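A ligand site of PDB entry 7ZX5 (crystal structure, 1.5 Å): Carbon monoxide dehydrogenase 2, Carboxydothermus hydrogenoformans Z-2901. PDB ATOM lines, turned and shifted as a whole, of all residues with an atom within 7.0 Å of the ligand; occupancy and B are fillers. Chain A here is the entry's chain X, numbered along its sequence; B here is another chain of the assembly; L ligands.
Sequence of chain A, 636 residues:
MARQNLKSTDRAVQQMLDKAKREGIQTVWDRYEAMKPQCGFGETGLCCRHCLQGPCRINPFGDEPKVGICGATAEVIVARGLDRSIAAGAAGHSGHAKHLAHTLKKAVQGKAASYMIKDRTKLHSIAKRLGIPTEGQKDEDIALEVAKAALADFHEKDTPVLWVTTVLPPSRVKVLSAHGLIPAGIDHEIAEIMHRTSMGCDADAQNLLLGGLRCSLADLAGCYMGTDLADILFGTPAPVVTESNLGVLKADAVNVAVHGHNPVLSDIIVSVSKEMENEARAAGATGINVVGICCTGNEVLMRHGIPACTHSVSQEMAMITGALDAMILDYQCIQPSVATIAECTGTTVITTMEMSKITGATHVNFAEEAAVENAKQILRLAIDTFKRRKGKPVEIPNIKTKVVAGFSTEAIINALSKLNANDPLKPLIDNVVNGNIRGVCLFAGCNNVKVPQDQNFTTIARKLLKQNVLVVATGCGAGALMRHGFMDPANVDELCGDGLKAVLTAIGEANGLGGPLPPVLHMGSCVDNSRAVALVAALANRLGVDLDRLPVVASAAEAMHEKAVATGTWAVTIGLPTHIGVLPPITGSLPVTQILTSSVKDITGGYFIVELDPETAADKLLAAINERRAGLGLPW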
ATOM      1  N   CYS A  47      14.823 -27.303 -26.091  1.00  0.00           N
ATOM      2  CA  CYS A  47      13.975 -26.331 -26.761  1.00  0.00           C
ATOM      3  C   CYS A  47      12.952 -27.088 -27.604  1.00  0.00           C
ATOM      4  O   CYS A  47      13.289 -28.103 -28.245  1.00  0.00           O
ATOM      5  CB  CYS A  47      14.790 -25.482 -27.693  1.00  0.00           C
ATOM      6  SG  CYS A  47      13.779 -24.258 -28.587  1.00  0.00           S
ATOM      7  N   CYS A  48      11.724 -26.554 -27.664  1.00  0.00           N
ATOM      8  CA  CYS A  48      10.680 -27.139 -28.517  1.00  0.00           C
ATOM      9  C   CYS A  48       9.925 -26.055 -29.247  1.00  0.00           C
ATOM     10  O   CYS A  48       9.574 -25.048 -28.622  1.00  0.00           O
ATOM     11  CB  CYS A  48       9.688 -27.937 -27.670  1.00  0.00           C
ATOM     12  SG  CYS A  48       8.339 -28.675 -28.567  1.00  0.00           S
ATOM     13  N   ARG A  49       9.756 -26.196 -30.556  1.00  0.00           N
ATOM     14  CA  ARG A  49       8.933 -25.324 -31.376  1.00  0.00           C
ATOM     15  C   ARG A  49       7.877 -26.128 -32.122  1.00  0.00           C
ATOM     16  O   ARG A  49       7.560 -25.815 -33.278  1.00  0.00           O
ATOM     17  CB  ARG A  49       9.798 -24.582 -32.363  1.00  0.00           C
ATOM     18  CG  ARG A  49      10.829 -23.753 -31.733  1.00  0.00           C
ATOM     19  CD  ARG A  49      11.875 -23.243 -32.687  1.00  0.00           C
ATOM     20  NE  ARG A  49      11.265 -22.503 -33.754  1.00  0.00           N
ATOM     21  CZ  ARG A  49      11.806 -22.296 -34.935  1.00  0.00           C
ATOM     22  NH1 ARG A  49      13.023 -22.687 -35.214  1.00  0.00           N
ATOM     23  NH2 ARG A  49      11.122 -21.616 -35.864  1.00  0.00           N
ATOM     24  N   HIS A  50       7.327 -27.207 -31.503  1.00  0.00           N
ATOM     25  CA  HIS A  50       6.403 -28.036 -32.200  1.00  0.00           C
ATOM     26  C   HIS A  50       4.964 -27.510 -32.168  1.00  0.00           C
ATOM     27  O   HIS A  50       4.117 -28.160 -32.793  1.00  0.00           O
ATOM     28  CB  HIS A  50       6.403 -29.475 -31.713  1.00  0.00           C
ATOM     29  CG  HIS A  50       7.712 -30.182 -31.885  1.00  0.00           C
ATOM     30  ND1 HIS A  50       7.794 -31.553 -31.755  1.00  0.00           N
ATOM     31  CD2 HIS A  50       8.932 -29.771 -32.315  1.00  0.00           C
ATOM     32  CE1 HIS A  50       9.042 -31.930 -31.985  1.00  0.00           C
ATOM     33  NE2 HIS A  50       9.760 -30.881 -32.350  1.00  0.00           N
ATOM     34  N   CYS A  51       4.697 -26.375 -31.565  1.00  0.00           N
ATOM     35  CA  CYS A  51       3.447 -25.703 -31.832  1.00  0.00           C
ATOM     36  C   CYS A  51       3.602 -24.197 -31.647  1.00  0.00           C
ATOM     37  O   CYS A  51       4.590 -23.713 -31.164  1.00  0.00           O
ATOM     38  CB  CYS A  51       2.300 -26.225 -30.937  1.00  0.00           C
ATOM     39  SG  CYS A  51       2.307 -25.574 -29.143  1.00  0.00           S
ATOM     40  N   LEU A  52       2.562 -23.471 -31.978  1.00  0.00           N
ATOM     41  CA  LEU A  52       2.652 -22.020 -31.974  1.00  0.00           C
ATOM     42  C   LEU A  52       2.448 -21.385 -30.591  1.00  0.00           C
ATOM     43  O   LEU A  52       2.415 -20.146 -30.471  1.00  0.00           O
ATOM     44  CB  LEU A  52       1.636 -21.414 -32.977  1.00  0.00           C
ATOM     45  CG  LEU A  52       1.907 -21.814 -34.452  1.00  0.00           C
ATOM     46  CD1 LEU A  52       0.850 -21.179 -35.343  1.00  0.00           C
ATOM     47  CD2 LEU A  52       3.228 -21.497 -34.968  1.00  0.00           C
ATOM     48  N   GLN A  53       2.330 -22.193 -29.539  1.00  0.00           N
ATOM     49  CA  GLN A  53       2.467 -21.671 -28.202  1.00  0.00           C
ATOM     50  C   GLN A  53       3.905 -21.447 -27.805  1.00  0.00           C
ATOM     51  O   GLN A  53       4.187 -20.688 -26.868  1.00  0.00           O
ATOM     52  CB  GLN A  53       1.827 -22.625 -27.218  1.00  0.00           C
ATOM     53  CG  GLN A  53       0.288 -22.617 -27.356  1.00  0.00           C
ATOM     54  CD  GLN A  53      -0.438 -23.556 -26.437  1.00  0.00           C
ATOM     55  OE1 GLN A  53       0.052 -24.664 -26.071  1.00  0.00           O
ATOM     56  NE2 GLN A  53      -1.606 -23.188 -26.075  1.00  0.00           N
ATOM     57  N   GLY A  54       4.795 -22.197 -28.426  1.00  0.00           N
ATOM     58  CA  GLY A  54       6.226 -22.043 -28.230  1.00  0.00           C
ATOM     59  C   GLY A  54       6.804 -20.759 -28.829  1.00  0.00           C
ATOM     60  O   GLY A  54       6.056 -19.891 -29.333  1.00  0.00           O
ATOM     61  N   PRO A  55       8.139 -20.597 -28.838  1.00  0.00           N
ATOM     62  CA  PRO A  55       9.158 -21.560 -28.441  1.00  0.00           C
ATOM     63  C   PRO A  55       9.107 -21.820 -26.927  1.00  0.00           C
ATOM     64  O   PRO A  55       8.916 -20.876 -26.137  1.00  0.00           O
ATOM     65  CB  PRO A  55      10.452 -20.847 -28.863  1.00  0.00           C
ATOM     66  CG  PRO A  55      10.113 -19.339 -28.672  1.00  0.00           C
ATOM     67  CD  PRO A  55       8.706 -19.261 -29.118  1.00  0.00           C
ATOM     68  N   CYS A  56       9.303 -23.064 -26.547  1.00  0.00           N
ATOM     69  CA  CYS A  56       9.411 -23.466 -25.165  1.00  0.00           C
ATOM     70  C   CYS A  56      10.874 -23.851 -24.959  1.00  0.00           C
ATOM     71  O   CYS A  56      11.528 -24.473 -25.842  1.00  0.00           O
ATOM     72  CB  CYS A  56       8.442 -24.580 -24.765  1.00  0.00           C
ATOM     73  SG  CYS A  56       6.776 -24.097 -24.723  1.00  0.00           S
ATOM     74  N   ARG A  57      11.387 -23.488 -23.819  1.00  0.00           N
ATOM     75  CA  ARG A  57      12.741 -23.917 -23.490  1.00  0.00           C
ATOM     76  C   ARG A  57      12.715 -24.318 -22.023  1.00  0.00           C
ATOM     77  O   ARG A  57      11.791 -23.976 -21.274  1.00  0.00           O
ATOM     78  CB  ARG A  57      13.726 -22.794 -23.757  1.00  0.00           C
ATOM     79  CG  ARG A  57      13.532 -21.664 -22.784  1.00  0.00           C
ATOM     80  CD  ARG A  57      14.193 -20.378 -23.046  1.00  0.00           C
ATOM     81  NE  ARG A  57      13.985 -19.489 -21.904  1.00  0.00           N
ATOM     82  CZ  ARG A  57      12.846 -18.835 -21.639  1.00  0.00           C
ATOM     83  NH1 ARG A  57      12.840 -18.084 -20.542  1.00  0.00           N
ATOM     84  NH2 ARG A  57      11.719 -18.891 -22.439  1.00  0.00           N
ATOM     85  N   VAL A  67       9.417 -26.793 -17.506  1.00  0.00           N
ATOM     86  CA  VAL A  67       8.510 -27.675 -18.217  1.00  0.00           C
ATOM     87  C   VAL A  67       7.910 -26.880 -19.358  1.00  0.00           C
ATOM     88  O   VAL A  67       7.745 -25.659 -19.285  1.00  0.00           O
ATOM     89  CB  VAL A  67       7.422 -28.226 -17.288  1.00  0.00           C
ATOM     90  CG1 VAL A  67       6.545 -27.126 -16.732  1.00  0.00           C
ATOM     91  CG2 VAL A  67       6.586 -29.263 -17.992  1.00  0.00           C
ATOM     92  N   GLY A  68       7.494 -27.595 -20.383  1.00  0.00           N
ATOM     93  CA  GLY A  68       6.820 -26.974 -21.520  1.00  0.00           C
ATOM     94  C   GLY A  68       5.441 -26.490 -21.184  1.00  0.00           C
ATOM     95  O   GLY A  68       4.852 -26.903 -20.213  1.00  0.00           O
ATOM     96  N   ILE A  69       4.945 -25.621 -22.072  1.00  0.00           N
ATOM     97  CA  ILE A  69       3.690 -24.953 -21.802  1.00  0.00           C
ATOM     98  C   ILE A  69       2.569 -25.993 -21.756  1.00  0.00           C
ATOM     99  O   ILE A  69       1.719 -25.948 -20.841  1.00  0.00           O
ATOM    100  CB  ILE A  69       3.433 -23.826 -22.836  1.00  0.00           C
ATOM    101  CG1 ILE A  69       4.393 -22.659 -22.628  1.00  0.00           C
ATOM    102  CG2 ILE A  69       1.984 -23.345 -22.741  1.00  0.00           C
ATOM    103  CD1 ILE A  69       4.357 -21.526 -23.673  1.00  0.00           C
ATOM    104  N   CYS A  70       2.656 -27.020 -22.616  1.00  0.00           N
ATOM    105  CA  CYS A  70       1.649 -28.065 -22.703  1.00  0.00           C
ATOM    106  C   CYS A  70       1.873 -29.133 -21.670  1.00  0.00           C
ATOM    107  O   CYS A  70       1.005 -30.001 -21.467  1.00  0.00           O
ATOM    108  CB  CYS A  70       1.720 -28.615 -24.089  1.00  0.00           C
ATOM    109  SG  CYS A  70       3.343 -29.448 -24.409  1.00  0.00           S
ATOM    110  N   GLY A  71       3.028 -29.049 -20.991  1.00  0.00           N
ATOM    111  CA  GLY A  71       3.381 -29.968 -19.915  1.00  0.00           C
ATOM    112  C   GLY A  71       4.422 -30.935 -20.313  1.00  0.00           C
ATOM    113  O   GLY A  71       4.758 -31.802 -19.495  1.00  0.00           O
ATOM    114  N   ALA A  72       4.949 -30.812 -21.535  1.00  0.00           N
ATOM    115  CA  ALA A  72       6.051 -31.643 -22.003  1.00  0.00           C
ATOM    116  C   ALA A  72       7.287 -31.484 -21.108  1.00  0.00           C
ATOM    117  O   ALA A  72       7.770 -30.383 -20.857  1.00  0.00           O
ATOM    118  CB  ALA A  72       6.405 -31.287 -23.436  1.00  0.00           C
ATOM    119  N   THR A  73       7.779 -32.616 -20.662  1.00  0.00           N
ATOM    120  CA  THR A  73       8.938 -32.642 -19.799  1.00  0.00           C
ATOM    121  C   THR A  73      10.217 -32.539 -20.623  1.00  0.00           C
ATOM    122  O   THR A  73      10.234 -32.698 -21.856  1.00  0.00           O
ATOM    123  CB  THR A  73       8.938 -33.908 -18.959  1.00  0.00           C
ATOM    124  OG1 THR A  73       9.082 -34.975 -19.875  1.00  0.00           O
ATOM    125  CG2 THR A  73       7.701 -34.074 -18.085  1.00  0.00           C
ATOM    126  N   ILE A  77      10.603 -33.577 -24.497  1.00  0.00           N
ATOM    127  CA  ILE A  77      11.140 -32.635 -25.486  1.00  0.00           C
ATOM    128  C   ILE A  77      12.421 -33.199 -26.140  1.00  0.00           C
ATOM    129  O   ILE A  77      12.607 -33.144 -27.386  1.00  0.00           O
ATOM    130  CB  ILE A  77      11.383 -31.276 -24.817  1.00  0.00           C
ATOM    131  CG1 ILE A  77      10.017 -30.623 -24.474  1.00  0.00           C
ATOM    132  CG2 ILE A  77      12.322 -30.399 -25.676  1.00  0.00           C
ATOM    133  CD1 ILE A  77      10.066 -29.327 -23.656  1.00  0.00           C
ATOM    134  N   ARG A  80      11.596 -36.205 -28.496  1.00  0.00           N
ATOM    135  CA  ARG A  80      10.864 -35.803 -29.701  1.00  0.00           C
ATOM    136  C   ARG A  80      11.761 -35.153 -30.714  1.00  0.00           C
ATOM    137  O   ARG A  80      11.687 -35.442 -31.919  1.00  0.00           O
ATOM    138  CB  ARG A  80       9.689 -34.837 -29.319  1.00  0.00           C
ATOM    139  CG  ARG A  80       8.608 -35.500 -28.531  1.00  0.00           C
ATOM    140  CD  ARG A  80       7.352 -34.696 -28.478  1.00  0.00           C
ATOM    141  NE  ARG A  80       7.584 -33.352 -27.939  1.00  0.00           N
ATOM    142  CZ  ARG A  80       6.614 -32.557 -27.510  1.00  0.00           C
ATOM    143  NH1 ARG A  80       5.394 -32.990 -27.531  1.00  0.00           N
ATOM    144  NH2 ARG A  80       6.869 -31.344 -27.046  1.00  0.00           N
ATOM    145  N   THR A 197       5.436 -37.172 -32.549  1.00  0.00           N
ATOM    146  CA  THR A 197       6.237 -36.103 -31.983  1.00  0.00           C
ATOM    147  C   THR A 197       5.584 -34.734 -32.070  1.00  0.00           C
ATOM    148  O   THR A 197       6.101 -33.783 -31.503  1.00  0.00           O
ATOM    149  CB  THR A 197       7.621 -36.041 -32.618  1.00  0.00           C
ATOM    150  OG1 THR A 197       7.536 -35.763 -34.016  1.00  0.00           O
ATOM    151  CG2 THR A 197       8.351 -37.337 -32.362  1.00  0.00           C
ATOM    152  N   SER A 198       4.404 -34.659 -32.724  1.00  0.00           N
ATOM    153  CA  SER A 198       3.634 -33.408 -32.746  1.00  0.00           C
ATOM    154  C   SER A 198       2.984 -33.163 -31.403  1.00  0.00           C
ATOM    155  O   SER A 198       2.937 -34.017 -30.510  1.00  0.00           O
ATOM    156  CB  SER A 198       2.646 -33.442 -33.919  1.00  0.00           C
ATOM    157  OG  SER A 198       1.512 -34.244 -33.712  1.00  0.00           O
ATOM    158  N   MET A 199       2.463 -31.942 -31.221  1.00  0.00           N
ATOM    159  CA  MET A 199       1.975 -31.544 -29.929  1.00  0.00           C
ATOM    160  C   MET A 199       0.818 -32.436 -29.444  1.00  0.00           C
ATOM    161  O   MET A 199      -0.150 -32.760 -30.186  1.00  0.00           O
ATOM    162  CB  MET A 199       1.551 -30.081 -30.022  1.00  0.00           C
ATOM    163  CG  MET A 199       1.020 -29.508 -28.747  1.00  0.00           C
ATOM    164  SD  MET A 199      -0.694 -29.886 -28.503  1.00  0.00           S
ATOM    165  CE  MET A 199      -1.192 -28.910 -27.045  1.00  0.00           C
ATOM    166  N   GLY A 200       0.905 -32.862 -28.189  1.00  0.00           N
ATOM    167  CA  GLY A 200      -0.178 -33.575 -27.577  1.00  0.00           C
ATOM    168  C   GLY A 200      -0.358 -34.988 -28.015  1.00  0.00           C
ATOM    169  O   GLY A 200      -1.449 -35.563 -27.926  1.00  0.00           O
ATOM    170  N   VAL B  28      -1.806 -24.716 -17.592  1.00  0.00           N
ATOM    171  CA  VAL B  28      -1.177 -24.261 -18.826  1.00  0.00           C
ATOM    172  C   VAL B  28      -0.848 -22.765 -18.775  1.00  0.00           C
ATOM    173  O   VAL B  28       0.187 -22.309 -19.313  1.00  0.00           O
ATOM    174  CB  VAL B  28      -2.051 -24.632 -20.034  1.00  0.00           C
ATOM    175  CG1 VAL B  28      -3.353 -23.921 -19.940  1.00  0.00           C
ATOM    176  CG2 VAL B  28      -1.361 -24.345 -21.289  1.00  0.00           C
ATOM    177  N   MET B  35       7.335 -19.179 -18.807  1.00  0.00           N
ATOM    178  CA  MET B  35       8.145 -19.254 -20.000  1.00  0.00           C
ATOM    179  C   MET B  35       8.504 -17.883 -20.515  1.00  0.00           C
ATOM    180  O   MET B  35       9.331 -17.760 -21.416  1.00  0.00           O
ATOM    181  CB  MET B  35       7.378 -20.041 -21.089  1.00  0.00           C
ATOM    182  CG  MET B  35       8.156 -20.535 -22.227  1.00  0.00           C
ATOM    183  SD  MET B  35       9.486 -21.673 -21.710  1.00  0.00           S
ATOM    184  CE  MET B  35       8.555 -23.113 -21.259  1.00  0.00           C
ATOM    185  N   GLN B  38       9.567 -15.236 -24.055  1.00  0.00           N
ATOM    186  CA  GLN B  38       9.902 -16.353 -24.930  1.00  0.00           C
ATOM    187  C   GLN B  38      10.969 -15.939 -25.950  1.00  0.00           C
ATOM    188  O   GLN B  38      11.227 -14.764 -26.209  1.00  0.00           O
ATOM    189  CB  GLN B  38       8.630 -16.842 -25.618  1.00  0.00           C
ATOM    190  CG  GLN B  38       7.630 -17.545 -24.679  1.00  0.00           C
ATOM    191  CD  GLN B  38       6.427 -18.061 -25.394  1.00  0.00           C
ATOM    192  OE1 GLN B  38       5.513 -17.282 -25.616  1.00  0.00           O
ATOM    193  NE2 GLN B  38       6.409 -19.328 -25.773  1.00  0.00           N
ATOM    194  N   PRO B 336       0.173 -33.198 -22.045  1.00  0.00           N
ATOM    195  CA  PRO B 336       0.670 -34.286 -21.195  1.00  0.00           C
ATOM    196  C   PRO B 336       0.605 -33.975 -19.691  1.00  0.00           C
ATOM    197  O   PRO B 336       0.671 -34.900 -18.868  1.00  0.00           O
ATOM    198  CB  PRO B 336       2.094 -34.522 -21.711  1.00  0.00           C
ATOM    199  CG  PRO B 336       2.512 -33.299 -22.457  1.00  0.00           C
ATOM    200  CD  PRO B 336       1.205 -32.697 -22.944  1.00  0.00           C
ATOM    201  N   MET B 560      -2.827 -23.052 -32.982  1.00  0.00           N
ATOM    202  CA  MET B 560      -1.717 -23.586 -32.180  1.00  0.00           C
ATOM    203  C   MET B 560      -0.948 -24.759 -32.835  1.00  0.00           C
ATOM    204  O   MET B 560       0.296 -24.732 -32.944  1.00  0.00           O
ATOM    205  CB  MET B 560      -2.305 -24.078 -30.874  1.00  0.00           C
ATOM    206  CG  MET B 560      -1.376 -24.731 -29.913  1.00  0.00           C
ATOM    207  SD  MET B 560      -1.277 -26.567 -29.923  1.00  0.00           S
ATOM    208  CE  MET B 560      -2.947 -27.034 -29.649  1.00  0.00           C
HETATM  209 FE1  LIG L   1       5.759 -25.760 -26.010  1.00  0.00          FE
HETATM  210 FE2  LIG L   1       4.110 -26.475 -28.093  1.00  0.00          FE
HETATM  211 FE3  LIG L   1       6.467 -27.749 -27.690  1.00  0.00          FE
HETATM  212 FE4  LIG L   1       4.379 -28.127 -25.824  1.00  0.00          FE
HETATM  213  S1  LIG L   1       4.452 -28.795 -28.159  1.00  0.00           S
HETATM  214  S2  LIG L   1       6.604 -27.853 -25.359  1.00  0.00           S
HETATM  215  S3  LIG L   1       3.509 -26.054 -25.834  1.00  0.00           S
HETATM  216  S4  LIG L   1       6.186 -25.561 -28.321  1.00  0.00           S
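FE4 of the ligand is bound by SG of Cys 70, at 2.2 Å.
The backbone NH of Gly 54 lies close to a sulfur (S4) of the ligand.
The backbone NH (N) of His 50 sits close to a sulfur (S4) of the ligand.
An iron atom (FE3) of the ligand is bound by the side-chain sulfur (SG) of Cys 48, 2.3 Å away.
SG of Cys 56 binds FE1 of the ligand (2.3 Å).
An iron atom (FE2) of the ligand is bound by the side-chain sulfur (SG) of Cys 51 (2.3 Å).
A sulfur (S3) of the ligand lies close to the side-chain amide oxygen of Gln 53 (3.7 Å).
A sulfur (S1) of the ligand lies close to the guanidinium group of Arg 80 (3.7 Å).
N of Cys 51 sits close to S4 of the ligand (3.7 Å).
N of Cys 70 sits close to S3 of the ligand (3.5 Å).
The side-chain sulfur (SG) of Cys 51 lies close to the side-chain sulfur (SD) of Met 560 of chain B (3.8 Å).
The side-chain sulfur (SG) of Cys 48 lies close to the guanidinium group (NH2) of Arg 80 (3.4 Å).
The side-chain sulfur (SG) of Cys 70 lies close to the backbone NH (N) of Ala 72.
O of Gln 53 is in hydrogen-bond range of NE2 of Gln 38 of chain B (2.8 Å).
The backbone carbonyl oxygen (O) of Thr 197 sits at hydrogen-bond distance from a ring nitrogen (ND1) of His 50 (2.8 Å).
The backbone carbonyl oxygen of Cys 56 sits close to the side-chain sulfur of Cys 47 (3.6 Å).
N of Ile 69 sits close to SG of Cys 56 (3.6 Å).
The side-chain sulfur of Cys 48 sits close to the backbone NH of His 50.
Residues that only touch the ligand: Met 199 (3.6 Å), Ile 69 (3.7 Å), Ala 72 (3.9 Å) and Gly 68 (3.9 Å).
Hydrophobic or aromatic side chains within 4 Å of the ligand: Ile 69, Ala 72 and Met 199.
Of the 29 residues printed, 12 come within 4 Å of the ligand.
The nearest printed residue that does not touch the ligand is Arg 49 (4.1 Å).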
